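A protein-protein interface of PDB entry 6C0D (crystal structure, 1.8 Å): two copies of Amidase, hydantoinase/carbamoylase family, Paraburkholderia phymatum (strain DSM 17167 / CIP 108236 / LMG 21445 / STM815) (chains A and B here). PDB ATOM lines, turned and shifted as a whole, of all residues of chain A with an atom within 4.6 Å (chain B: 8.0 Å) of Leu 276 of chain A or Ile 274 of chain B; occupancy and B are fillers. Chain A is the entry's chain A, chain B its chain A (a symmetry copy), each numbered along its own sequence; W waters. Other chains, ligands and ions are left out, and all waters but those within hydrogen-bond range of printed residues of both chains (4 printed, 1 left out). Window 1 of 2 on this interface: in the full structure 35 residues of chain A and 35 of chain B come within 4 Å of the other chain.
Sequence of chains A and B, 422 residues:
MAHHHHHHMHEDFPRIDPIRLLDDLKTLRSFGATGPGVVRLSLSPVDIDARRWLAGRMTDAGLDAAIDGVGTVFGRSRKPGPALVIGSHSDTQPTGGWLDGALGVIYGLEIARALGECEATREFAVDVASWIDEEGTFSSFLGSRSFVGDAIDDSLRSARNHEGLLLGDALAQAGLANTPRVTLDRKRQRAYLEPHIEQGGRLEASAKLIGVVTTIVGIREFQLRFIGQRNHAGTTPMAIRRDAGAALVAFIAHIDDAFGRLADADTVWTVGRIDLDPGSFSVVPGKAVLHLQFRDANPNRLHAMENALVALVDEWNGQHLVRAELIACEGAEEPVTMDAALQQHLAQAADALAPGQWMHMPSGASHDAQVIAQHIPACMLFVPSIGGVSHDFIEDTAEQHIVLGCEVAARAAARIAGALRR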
ATOM      1  N   GLY A 245      13.652 -16.747 -24.953  1.00  0.00           N
ATOM      2  CA  GLY A 245      13.215 -18.082 -24.550  1.00  0.00           C
ATOM      3  C   GLY A 245      13.516 -19.133 -25.600  1.00  0.00           C
ATOM      4  O   GLY A 245      13.822 -20.282 -25.273  1.00  0.00           O
ATOM      5  N   VAL A 249      15.897 -22.513 -25.000  1.00  0.00           N
ATOM      6  CA  VAL A 249      15.486 -23.883 -25.300  1.00  0.00           C
ATOM      7  C   VAL A 249      16.478 -24.540 -26.249  1.00  0.00           C
ATOM      8  O   VAL A 249      16.836 -25.718 -26.110  1.00  0.00           O
ATOM      9  CB  VAL A 249      14.055 -23.860 -25.881  1.00  0.00           C
ATOM     10  CG1 VAL A 249      13.751 -25.111 -26.682  1.00  0.00           C
ATOM     11  CG2 VAL A 249      13.037 -23.649 -24.770  1.00  0.00           C
ATOM     12  N   ILE A 274      13.247 -22.675 -15.252  1.00  0.00           N
ATOM     13  CA  ILE A 274      13.281 -21.827 -16.447  1.00  0.00           C
ATOM     14  C   ILE A 274      12.314 -20.667 -16.224  1.00  0.00           C
ATOM     15  O   ILE A 274      11.173 -20.887 -15.809  1.00  0.00           O
ATOM     16  CB  ILE A 274      12.879 -22.617 -17.713  1.00  0.00           C
ATOM     17  CG1 ILE A 274      13.920 -23.689 -18.050  1.00  0.00           C
ATOM     18  CG2 ILE A 274      12.655 -21.668 -18.927  1.00  0.00           C
ATOM     19  CD1 ILE A 274      13.425 -24.656 -19.168  1.00  0.00           C
ATOM     20  N   ASP A 275      12.760 -19.434 -16.492  1.00  0.00           N
ATOM     21  CA  ASP A 275      11.922 -18.249 -16.337  1.00  0.00           C
ATOM     22  C   ASP A 275      12.054 -17.396 -17.589  1.00  0.00           C
ATOM     23  O   ASP A 275      13.173 -17.056 -17.989  1.00  0.00           O
ATOM     24  CB  ASP A 275      12.326 -17.412 -15.104  1.00  0.00           C
ATOM     25  CG  ASP A 275      12.157 -18.170 -13.782  1.00  0.00           C
ATOM     26  OD1 ASP A 275      11.022 -18.579 -13.468  1.00  0.00           O
ATOM     27  OD2 ASP A 275      13.161 -18.349 -13.052  1.00  0.00           O
ATOM     28  N   LEU A 276      10.924 -17.068 -18.214  1.00  0.00           N
ATOM     29  CA  LEU A 276      10.888 -16.154 -19.348  1.00  0.00           C
ATOM     30  C   LEU A 276      10.310 -14.819 -18.895  1.00  0.00           C
ATOM     31  O   LEU A 276       9.362 -14.774 -18.102  1.00  0.00           O
ATOM     32  CB  LEU A 276      10.043 -16.695 -20.518  1.00  0.00           C
ATOM     33  CG  LEU A 276      10.270 -18.137 -20.979  1.00  0.00           C
ATOM     34  CD1 LEU A 276       9.523 -18.430 -22.301  1.00  0.00           C
ATOM     35  CD2 LEU A 276      11.740 -18.512 -21.080  1.00  0.00           C
ATOM     36  N   ASP A 277      10.892 -13.738 -19.409  1.00  0.00           N
ATOM     37  CA  ASP A 277      10.478 -12.389 -19.057  1.00  0.00           C
ATOM     38  C   ASP A 277       9.946 -11.694 -20.304  1.00  0.00           C
ATOM     39  O   ASP A 277      10.667 -11.592 -21.308  1.00  0.00           O
ATOM     40  CB  ASP A 277      11.646 -11.609 -18.454  1.00  0.00           C
ATOM     41  CG  ASP A 277      11.265 -10.201 -18.087  1.00  0.00           C
ATOM     42  OD1 ASP A 277      11.578  -9.275 -18.866  1.00  0.00           O
ATOM     43  OD2 ASP A 277      10.626 -10.031 -17.031  1.00  0.00           O
ATOM     44  N   PRO A 278       8.710 -11.173 -20.309  1.00  0.00           N
ATOM     45  CA  PRO A 278       7.904 -11.050 -19.086  1.00  0.00           C
ATOM     46  C   PRO A 278       7.019 -12.235 -18.744  1.00  0.00           C
ATOM     47  O   PRO A 278       6.458 -12.253 -17.639  1.00  0.00           O
ATOM     48  CB  PRO A 278       7.024  -9.826 -19.396  1.00  0.00           C
ATOM     49  CG  PRO A 278       6.804  -9.904 -20.883  1.00  0.00           C
ATOM     50  CD  PRO A 278       8.117 -10.439 -21.450  1.00  0.00           C
ATOM     51  N   GLY A 279       6.868 -13.206 -19.642  1.00  0.00           N
ATOM     52  CA  GLY A 279       6.072 -14.383 -19.338  1.00  0.00           C
ATOM     53  C   GLY A 279       4.603 -14.208 -19.678  1.00  0.00           C
ATOM     54  O   GLY A 279       3.739 -14.705 -18.952  1.00  0.00           O
ATOM     55  N   PRO A 285       9.639 -13.023 -25.446  1.00  0.00           N
ATOM     56  CA  PRO A 285      10.470 -12.762 -24.255  1.00  0.00           C
ATOM     57  C   PRO A 285      11.776 -12.076 -24.624  1.00  0.00           C
ATOM     58  O   PRO A 285      12.519 -12.554 -25.481  1.00  0.00           O
ATOM     59  CB  PRO A 285      10.735 -14.164 -23.681  1.00  0.00           C
ATOM     60  CG  PRO A 285       9.713 -15.073 -24.305  1.00  0.00           C
ATOM     61  CD  PRO A 285       9.347 -14.454 -25.640  1.00  0.00           C
ATOM     62  N   LYS A 287      14.143 -11.509 -22.216  1.00  0.00           N
ATOM     63  CA  LYS A 287      15.125 -12.112 -21.321  1.00  0.00           C
ATOM     64  C   LYS A 287      14.621 -13.475 -20.880  1.00  0.00           C
ATOM     65  O   LYS A 287      13.412 -13.715 -20.822  1.00  0.00           O
ATOM     66  CB  LYS A 287      15.399 -11.253 -20.076  1.00  0.00           C
ATOM     67  CG  LYS A 287      16.019  -9.890 -20.370  1.00  0.00           C
ATOM     68  CD  LYS A 287      16.259  -9.100 -19.078  1.00  0.00           C
ATOM     69  CE  LYS A 287      16.874  -7.731 -19.374  1.00  0.00           C
ATOM     70  NZ  LYS A 287      16.994  -6.877 -18.149  1.00  0.00           N
ATOM     71  N   ALA A 288      15.561 -14.358 -20.542  1.00  0.00           N
ATOM     72  CA  ALA A 288      15.237 -15.705 -20.099  1.00  0.00           C
ATOM     73  C   ALA A 288      16.408 -16.220 -19.271  1.00  0.00           C
ATOM     74  O   ALA A 288      17.565 -15.882 -19.544  1.00  0.00           O
ATOM     75  CB  ALA A 288      14.972 -16.637 -21.282  1.00  0.00           C
ATOM     76  N   LEU B 224       0.127 -26.059 -22.823  1.00  0.00           N
ATOM     77  CA  LEU B 224       0.573 -27.428 -23.010  1.00  0.00           C
ATOM     78  C   LEU B 224       1.247 -27.868 -21.722  1.00  0.00           C
ATOM     79  O   LEU B 224       2.263 -27.282 -21.318  1.00  0.00           O
ATOM     80  CB  LEU B 224       1.517 -27.522 -24.200  1.00  0.00           C
ATOM     81  CG  LEU B 224       1.977 -28.920 -24.570  1.00  0.00           C
ATOM     82  CD1 LEU B 224       0.799 -29.816 -24.948  1.00  0.00           C
ATOM     83  CD2 LEU B 224       2.902 -28.751 -25.718  1.00  0.00           C
ATOM     84  N   ALA B 244       9.779 -33.542 -16.598  1.00  0.00           N
ATOM     85  CA  ALA B 244       8.738 -32.848 -17.355  1.00  0.00           C
ATOM     86  C   ALA B 244       9.287 -31.634 -18.094  1.00  0.00           C
ATOM     87  O   ALA B 244       8.750 -31.252 -19.144  1.00  0.00           O
ATOM     88  CB  ALA B 244       7.613 -32.412 -16.418  1.00  0.00           C
ATOM     89  N   GLY B 245      10.305 -30.979 -17.538  1.00  0.00           N
ATOM     90  CA  GLY B 245      10.880 -29.825 -18.225  1.00  0.00           C
ATOM     91  C   GLY B 245      11.685 -30.217 -19.449  1.00  0.00           C
ATOM     92  O   GLY B 245      11.705 -29.496 -20.448  1.00  0.00           O
ATOM     93  N   LEU B 248       9.181 -30.825 -22.110  1.00  0.00           N
ATOM     94  CA  LEU B 248       8.659 -29.563 -22.633  1.00  0.00           C
ATOM     95  C   LEU B 248       9.607 -28.966 -23.665  1.00  0.00           C
ATOM     96  O   LEU B 248       9.178 -28.500 -24.732  1.00  0.00           O
ATOM     97  CB  LEU B 248       8.442 -28.585 -21.474  1.00  0.00           C
ATOM     98  CG  LEU B 248       7.881 -27.190 -21.796  1.00  0.00           C
ATOM     99  CD1 LEU B 248       7.187 -26.615 -20.566  1.00  0.00           C
ATOM    100  CD2 LEU B 248       8.986 -26.212 -22.247  1.00  0.00           C
ATOM    101  N   VAL B 249      10.907 -28.933 -23.347  1.00  0.00           N
ATOM    102  CA  VAL B 249      11.894 -28.315 -24.231  1.00  0.00           C
ATOM    103  C   VAL B 249      11.998 -29.091 -25.536  1.00  0.00           C
ATOM    104  O   VAL B 249      12.105 -28.519 -26.630  1.00  0.00           O
ATOM    105  CB  VAL B 249      13.249 -28.238 -23.492  1.00  0.00           C
ATOM    106  CG1 VAL B 249      14.411 -28.109 -24.456  1.00  0.00           C
ATOM    107  CG2 VAL B 249      13.235 -27.101 -22.480  1.00  0.00           C
ATOM    108  N   ILE B 252       9.039 -28.292 -27.812  1.00  0.00           N
ATOM    109  CA  ILE B 252       9.070 -27.022 -28.532  1.00  0.00           C
ATOM    110  C   ILE B 252       9.767 -27.198 -29.872  1.00  0.00           C
ATOM    111  O   ILE B 252       9.346 -26.621 -30.883  1.00  0.00           O
ATOM    112  CB  ILE B 252       9.729 -25.923 -27.675  1.00  0.00           C
ATOM    113  CG1 ILE B 252       8.794 -25.533 -26.523  1.00  0.00           C
ATOM    114  CG2 ILE B 252      10.045 -24.662 -28.537  1.00  0.00           C
ATOM    115  CD1 ILE B 252       9.438 -24.537 -25.490  1.00  0.00           C
ATOM    116  N   THR B 270       4.702 -18.180 -30.890  1.00  0.00           N
ATOM    117  CA  THR B 270       5.455 -17.654 -29.748  1.00  0.00           C
ATOM    118  C   THR B 270       5.201 -18.504 -28.522  1.00  0.00           C
ATOM    119  O   THR B 270       4.045 -18.733 -28.164  1.00  0.00           O
ATOM    120  CB  THR B 270       5.030 -16.211 -29.424  1.00  0.00           C
ATOM    121  OG1 THR B 270       4.906 -15.456 -30.635  1.00  0.00           O
ATOM    122  CG2 THR B 270       6.061 -15.534 -28.502  1.00  0.00           C
ATOM    123  N   VAL B 271       6.275 -18.913 -27.855  1.00  0.00           N
ATOM    124  CA  VAL B 271       6.179 -19.491 -26.518  1.00  0.00           C
ATOM    125  C   VAL B 271       6.435 -18.341 -25.549  1.00  0.00           C
ATOM    126  O   VAL B 271       7.584 -17.907 -25.361  1.00  0.00           O
ATOM    127  CB  VAL B 271       7.174 -20.637 -26.324  1.00  0.00           C
ATOM    128  CG1 VAL B 271       7.191 -21.084 -24.847  1.00  0.00           C
ATOM    129  CG2 VAL B 271       6.807 -21.819 -27.244  1.00  0.00           C
ATOM    130  N   GLY B 272       5.367 -17.842 -24.924  1.00  0.00           N
ATOM    131  CA  GLY B 272       5.513 -16.659 -24.103  1.00  0.00           C
ATOM    132  C   GLY B 272       5.837 -16.942 -22.652  1.00  0.00           C
ATOM    133  O   GLY B 272       6.294 -16.053 -21.924  1.00  0.00           O
ATOM    134  N   ARG B 273       5.611 -18.176 -22.219  1.00  0.00           N
ATOM    135  CA  ARG B 273       5.824 -18.521 -20.821  1.00  0.00           C
ATOM    136  C   ARG B 273       6.177 -19.995 -20.701  1.00  0.00           C
ATOM    137  O   ARG B 273       5.639 -20.829 -21.439  1.00  0.00           O
ATOM    138  CB  ARG B 273       4.572 -18.217 -19.990  1.00  0.00           C
ATOM    139  CG  ARG B 273       4.800 -18.283 -18.492  1.00  0.00           C
ATOM    140  CD  ARG B 273       3.503 -18.028 -17.706  1.00  0.00           C
ATOM    141  NE  ARG B 273       3.773 -17.982 -16.269  1.00  0.00           N
ATOM    142  CZ  ARG B 273       4.015 -16.862 -15.592  1.00  0.00           C
ATOM    143  NH1 ARG B 273       4.000 -15.690 -16.217  1.00  0.00           N
ATOM    144  NH2 ARG B 273       4.269 -16.915 -14.292  1.00  0.00           N
ATOM    145  N   ILE B 274       7.075 -20.300 -19.761  1.00  0.00           N
ATOM    146  CA  ILE B 274       7.440 -21.669 -19.387  1.00  0.00           C
ATOM    147  C   ILE B 274       7.559 -21.721 -17.866  1.00  0.00           C
ATOM    148  O   ILE B 274       8.208 -20.859 -17.269  1.00  0.00           O
ATOM    149  CB  ILE B 274       8.774 -22.098 -20.039  1.00  0.00           C
ATOM    150  CG1 ILE B 274       8.637 -22.207 -21.560  1.00  0.00           C
ATOM    151  CG2 ILE B 274       9.296 -23.436 -19.437  1.00  0.00           C
ATOM    152  CD1 ILE B 274      10.017 -22.395 -22.261  1.00  0.00           C
ATOM    153  N   ASP B 275       6.936 -22.723 -17.234  1.00  0.00           N
ATOM    154  CA  ASP B 275       6.994 -22.889 -15.785  1.00  0.00           C
ATOM    155  C   ASP B 275       7.321 -24.342 -15.478  1.00  0.00           C
ATOM    156  O   ASP B 275       6.634 -25.247 -15.965  1.00  0.00           O
ATOM    157  CB  ASP B 275       5.661 -22.511 -15.106  1.00  0.00           C
ATOM    158  CG  ASP B 275       5.282 -21.037 -15.302  1.00  0.00           C
ATOM    159  OD1 ASP B 275       6.059 -20.159 -14.877  1.00  0.00           O
ATOM    160  OD2 ASP B 275       4.202 -20.761 -15.876  1.00  0.00           O
ATOM    161  N   LEU B 276       8.373 -24.567 -14.689  1.00  0.00           N
ATOM    162  CA  LEU B 276       8.727 -25.895 -14.210  1.00  0.00           C
ATOM    163  C   LEU B 276       8.366 -26.005 -12.733  1.00  0.00           C
ATOM    164  O   LEU B 276       8.554 -25.057 -11.963  1.00  0.00           O
ATOM    165  CB  LEU B 276      10.225 -26.210 -14.385  1.00  0.00           C
ATOM    166  CG  LEU B 276      10.880 -25.920 -15.738  1.00  0.00           C
ATOM    167  CD1 LEU B 276      12.306 -26.514 -15.812  1.00  0.00           C
ATOM    168  CD2 LEU B 276      10.035 -26.361 -16.922  1.00  0.00           C
ATOM    169  N   ASP B 277       7.850 -27.172 -12.354  1.00  0.00           N
ATOM    170  CA  ASP B 277       7.427 -27.428 -10.986  1.00  0.00           C
ATOM    171  C   ASP B 277       8.283 -28.547 -10.405  1.00  0.00           C
ATOM    172  O   ASP B 277       8.328 -29.648 -10.974  1.00  0.00           O
ATOM    173  CB  ASP B 277       5.944 -27.797 -10.941  1.00  0.00           C
ATOM    174  CG  ASP B 277       5.468 -28.085  -9.544  1.00  0.00           C
ATOM    175  OD1 ASP B 277       5.359 -29.276  -9.184  1.00  0.00           O
ATOM    176  OD2 ASP B 277       5.232 -27.112  -8.802  1.00  0.00           O
ATOM    177  N   ALA B 288       5.431 -29.494 -15.850  1.00  0.00           N
ATOM    178  CA  ALA B 288       5.907 -28.345 -16.606  1.00  0.00           C
ATOM    179  C   ALA B 288       4.777 -27.882 -17.516  1.00  0.00           C
ATOM    180  O   ALA B 288       3.988 -28.702 -18.000  1.00  0.00           O
ATOM    181  CB  ALA B 288       7.148 -28.687 -17.429  1.00  0.00           C
ATOM    182  N   VAL B 289       4.710 -26.577 -17.770  1.00  0.00           N
ATOM    183  CA  VAL B 289       3.667 -26.024 -18.633  1.00  0.00           C
ATOM    184  C   VAL B 289       4.260 -24.905 -19.474  1.00  0.00           C
ATOM    185  O   VAL B 289       5.098 -24.125 -19.002  1.00  0.00           O
ATOM    186  CB  VAL B 289       2.452 -25.532 -17.806  1.00  0.00           C
ATOM    187  CG1 VAL B 289       2.877 -24.459 -16.824  1.00  0.00           C
ATOM    188  CG2 VAL B 289       1.334 -25.004 -18.732  1.00  0.00           C
ATOM    189  N   LEU B 290       3.853 -24.848 -20.742  1.00  0.00           N
ATOM    190  CA  LEU B 290       4.205 -23.716 -21.583  1.00  0.00           C
ATOM    191  C   LEU B 290       2.920 -23.071 -22.081  1.00  0.00           C
ATOM    192  O   LEU B 290       1.874 -23.722 -22.170  1.00  0.00           O
ATOM    193  CB  LEU B 290       5.103 -24.116 -22.775  1.00  0.00           C
ATOM    194  CG  LEU B 290       4.574 -25.022 -23.908  1.00  0.00           C
ATOM    195  CD1 LEU B 290       3.645 -24.270 -24.912  1.00  0.00           C
ATOM    196  CD2 LEU B 290       5.746 -25.604 -24.665  1.00  0.00           C
ATOM    197  N   HIS B 291       3.011 -21.790 -22.399  1.00  0.00           N
ATOM    198  CA  HIS B 291       1.946 -21.064 -23.073  1.00  0.00           C
ATOM    199  C   HIS B 291       2.374 -20.811 -24.513  1.00  0.00           C
ATOM    200  O   HIS B 291       3.494 -20.336 -24.756  1.00  0.00           O
ATOM    201  CB  HIS B 291       1.654 -19.748 -22.350  1.00  0.00           C
ATOM    202  CG  HIS B 291       1.171 -19.933 -20.943  1.00  0.00           C
ATOM    203  ND1 HIS B 291       0.515 -18.944 -20.243  1.00  0.00           N
ATOM    204  CD2 HIS B 291       1.249 -20.995 -20.108  1.00  0.00           C
ATOM    205  CE1 HIS B 291       0.196 -19.397 -19.042  1.00  0.00           C
ATOM    206  NE2 HIS B 291       0.629 -20.638 -18.936  1.00  0.00           N
HETATM  207  O   HOH W   1      10.390 -22.699 -14.038  1.00  0.00           O
HETATM  208  O   HOH W   2       8.398 -18.270 -17.820  1.00  0.00           O
HETATM  209  O   HOH W   3       7.298 -16.479 -16.300  1.00  0.00           O
HETATM  210  O   HOH W   4       6.755 -13.419 -22.563  1.00  0.00           O
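O of Gly 279 of chain A lies within hydrogen-bond range of NH1 of Arg 273 of chain B, at 2.9 Å. O of Ile 274 of chain B lies close to O of Ile 274 of chain A, at 3.3 Å.
The backbone carbonyl oxygen (O) of His 291 of chain B lies within hydrogen-bond range of the backbone NH (N) of Gly 272 of chain B (3.1 Å). The guanidinium group of Arg 273 of chain B is in salt-bridge range of the side-chain carboxylate of Asp 275 of chain B (2.8 Å). The backbone carbonyl oxygen of Arg 273 of chain B lies within hydrogen-bond range of the backbone NH of His 291 of chain B, at 3.0 Å.
CG1 of Val 249 of chain A touches O of Val 249 of chain B, 3.8 Å away. Ile 252 of chain B touches Val 249 of chain A. Ile 274 of chain A touches Leu 276 of chain B. O of Val 271 of chain B touches CD1 of Leu 276 of chain A, at 3.7 Å. CD1 of Leu 276 of chain A touches C of Gly 272 of chain B, at 3.99 Å. N of Arg 273 of chain B touches CD1 of Leu 276 of chain A, at 3.9 Å. Leu 276 of chain A touches Ile 274 of chain B. Gly 279 of chain A touches Gly 272 of chain B (CA to O, 3.1 Å). CG of Pro 285 of chain A touches O of Val 271 of chain B, at 3.7 Å.
Of the printed residues of chain B, Leu 276 of chain A touches Val 271, Gly 272, Arg 273 and Ile 274. Of the printed residues of chain A, Ile 274 of chain B touches Ile 274 and Leu 276. Of the printed residues of chain B, Pro 285 of chain A touches Val 271. Of the printed residues of chain B, Val 249 of chain A touches Val 249 and Ile 252. Printed residues of chain A within 4 Å of Arg 273 of chain B: Leu 276 and Gly 279. His 291 of chain B touches none of the printed residues of chain A. Ala 244 of chain B touches none of the printed residues of chain A. The nearest printed residue of chain B that does not touch Leu 276 of chain A is Asp 275 of chain B (6.7 Å). The nearest printed residue of chain A that does not touch Ile 274 of chain B is Val 249 of chain A (4.1 Å). The nearest printed residue of chain A that does not touch Val 249 of chain B is Ile 274 of chain A (4.1 Å).
Hydrophobic or aromatic side chains of chain A within 4 Å of the printed part of chain B: Val 249, Ile 274, Leu 276 and Pro 285. Among the printed residues, 11 pairs touch across the chains. Among the printed residues, no Asp or Glu carboxylate lies within 4 Å of a Lys or Arg side-chain nitrogen of the other chain.
Val 249 of chain B touches its own counterpart, Val 249 of chain A. Ile 274 of chain A touches its own counterpart, Ile 274 of chain B. Ile 274 of chain A touches Leu 276 of chain B, and with the chains exchanged Leu 276 of chain A touches Ile 274 of chain B.
Water W1 bridges O of Ile 274 of chain A (2.7 Å) and N of Leu 276 of chain B (2.8 Å). Water W2 bridges O of Ile 274 of chain B (2.7 Å) and N of Leu 276 of chain A (2.8 Å). Water W4 bridges O of Gly 272 of chain B (2.7 Å) and N of Gly 279 of chain A (2.9 Å). Water W3 bridges the backbone carbonyl oxygen of Leu 276 of chain A (3.2 Å) and the guanidinium group of Arg 273 of chain B (3.4 Å).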
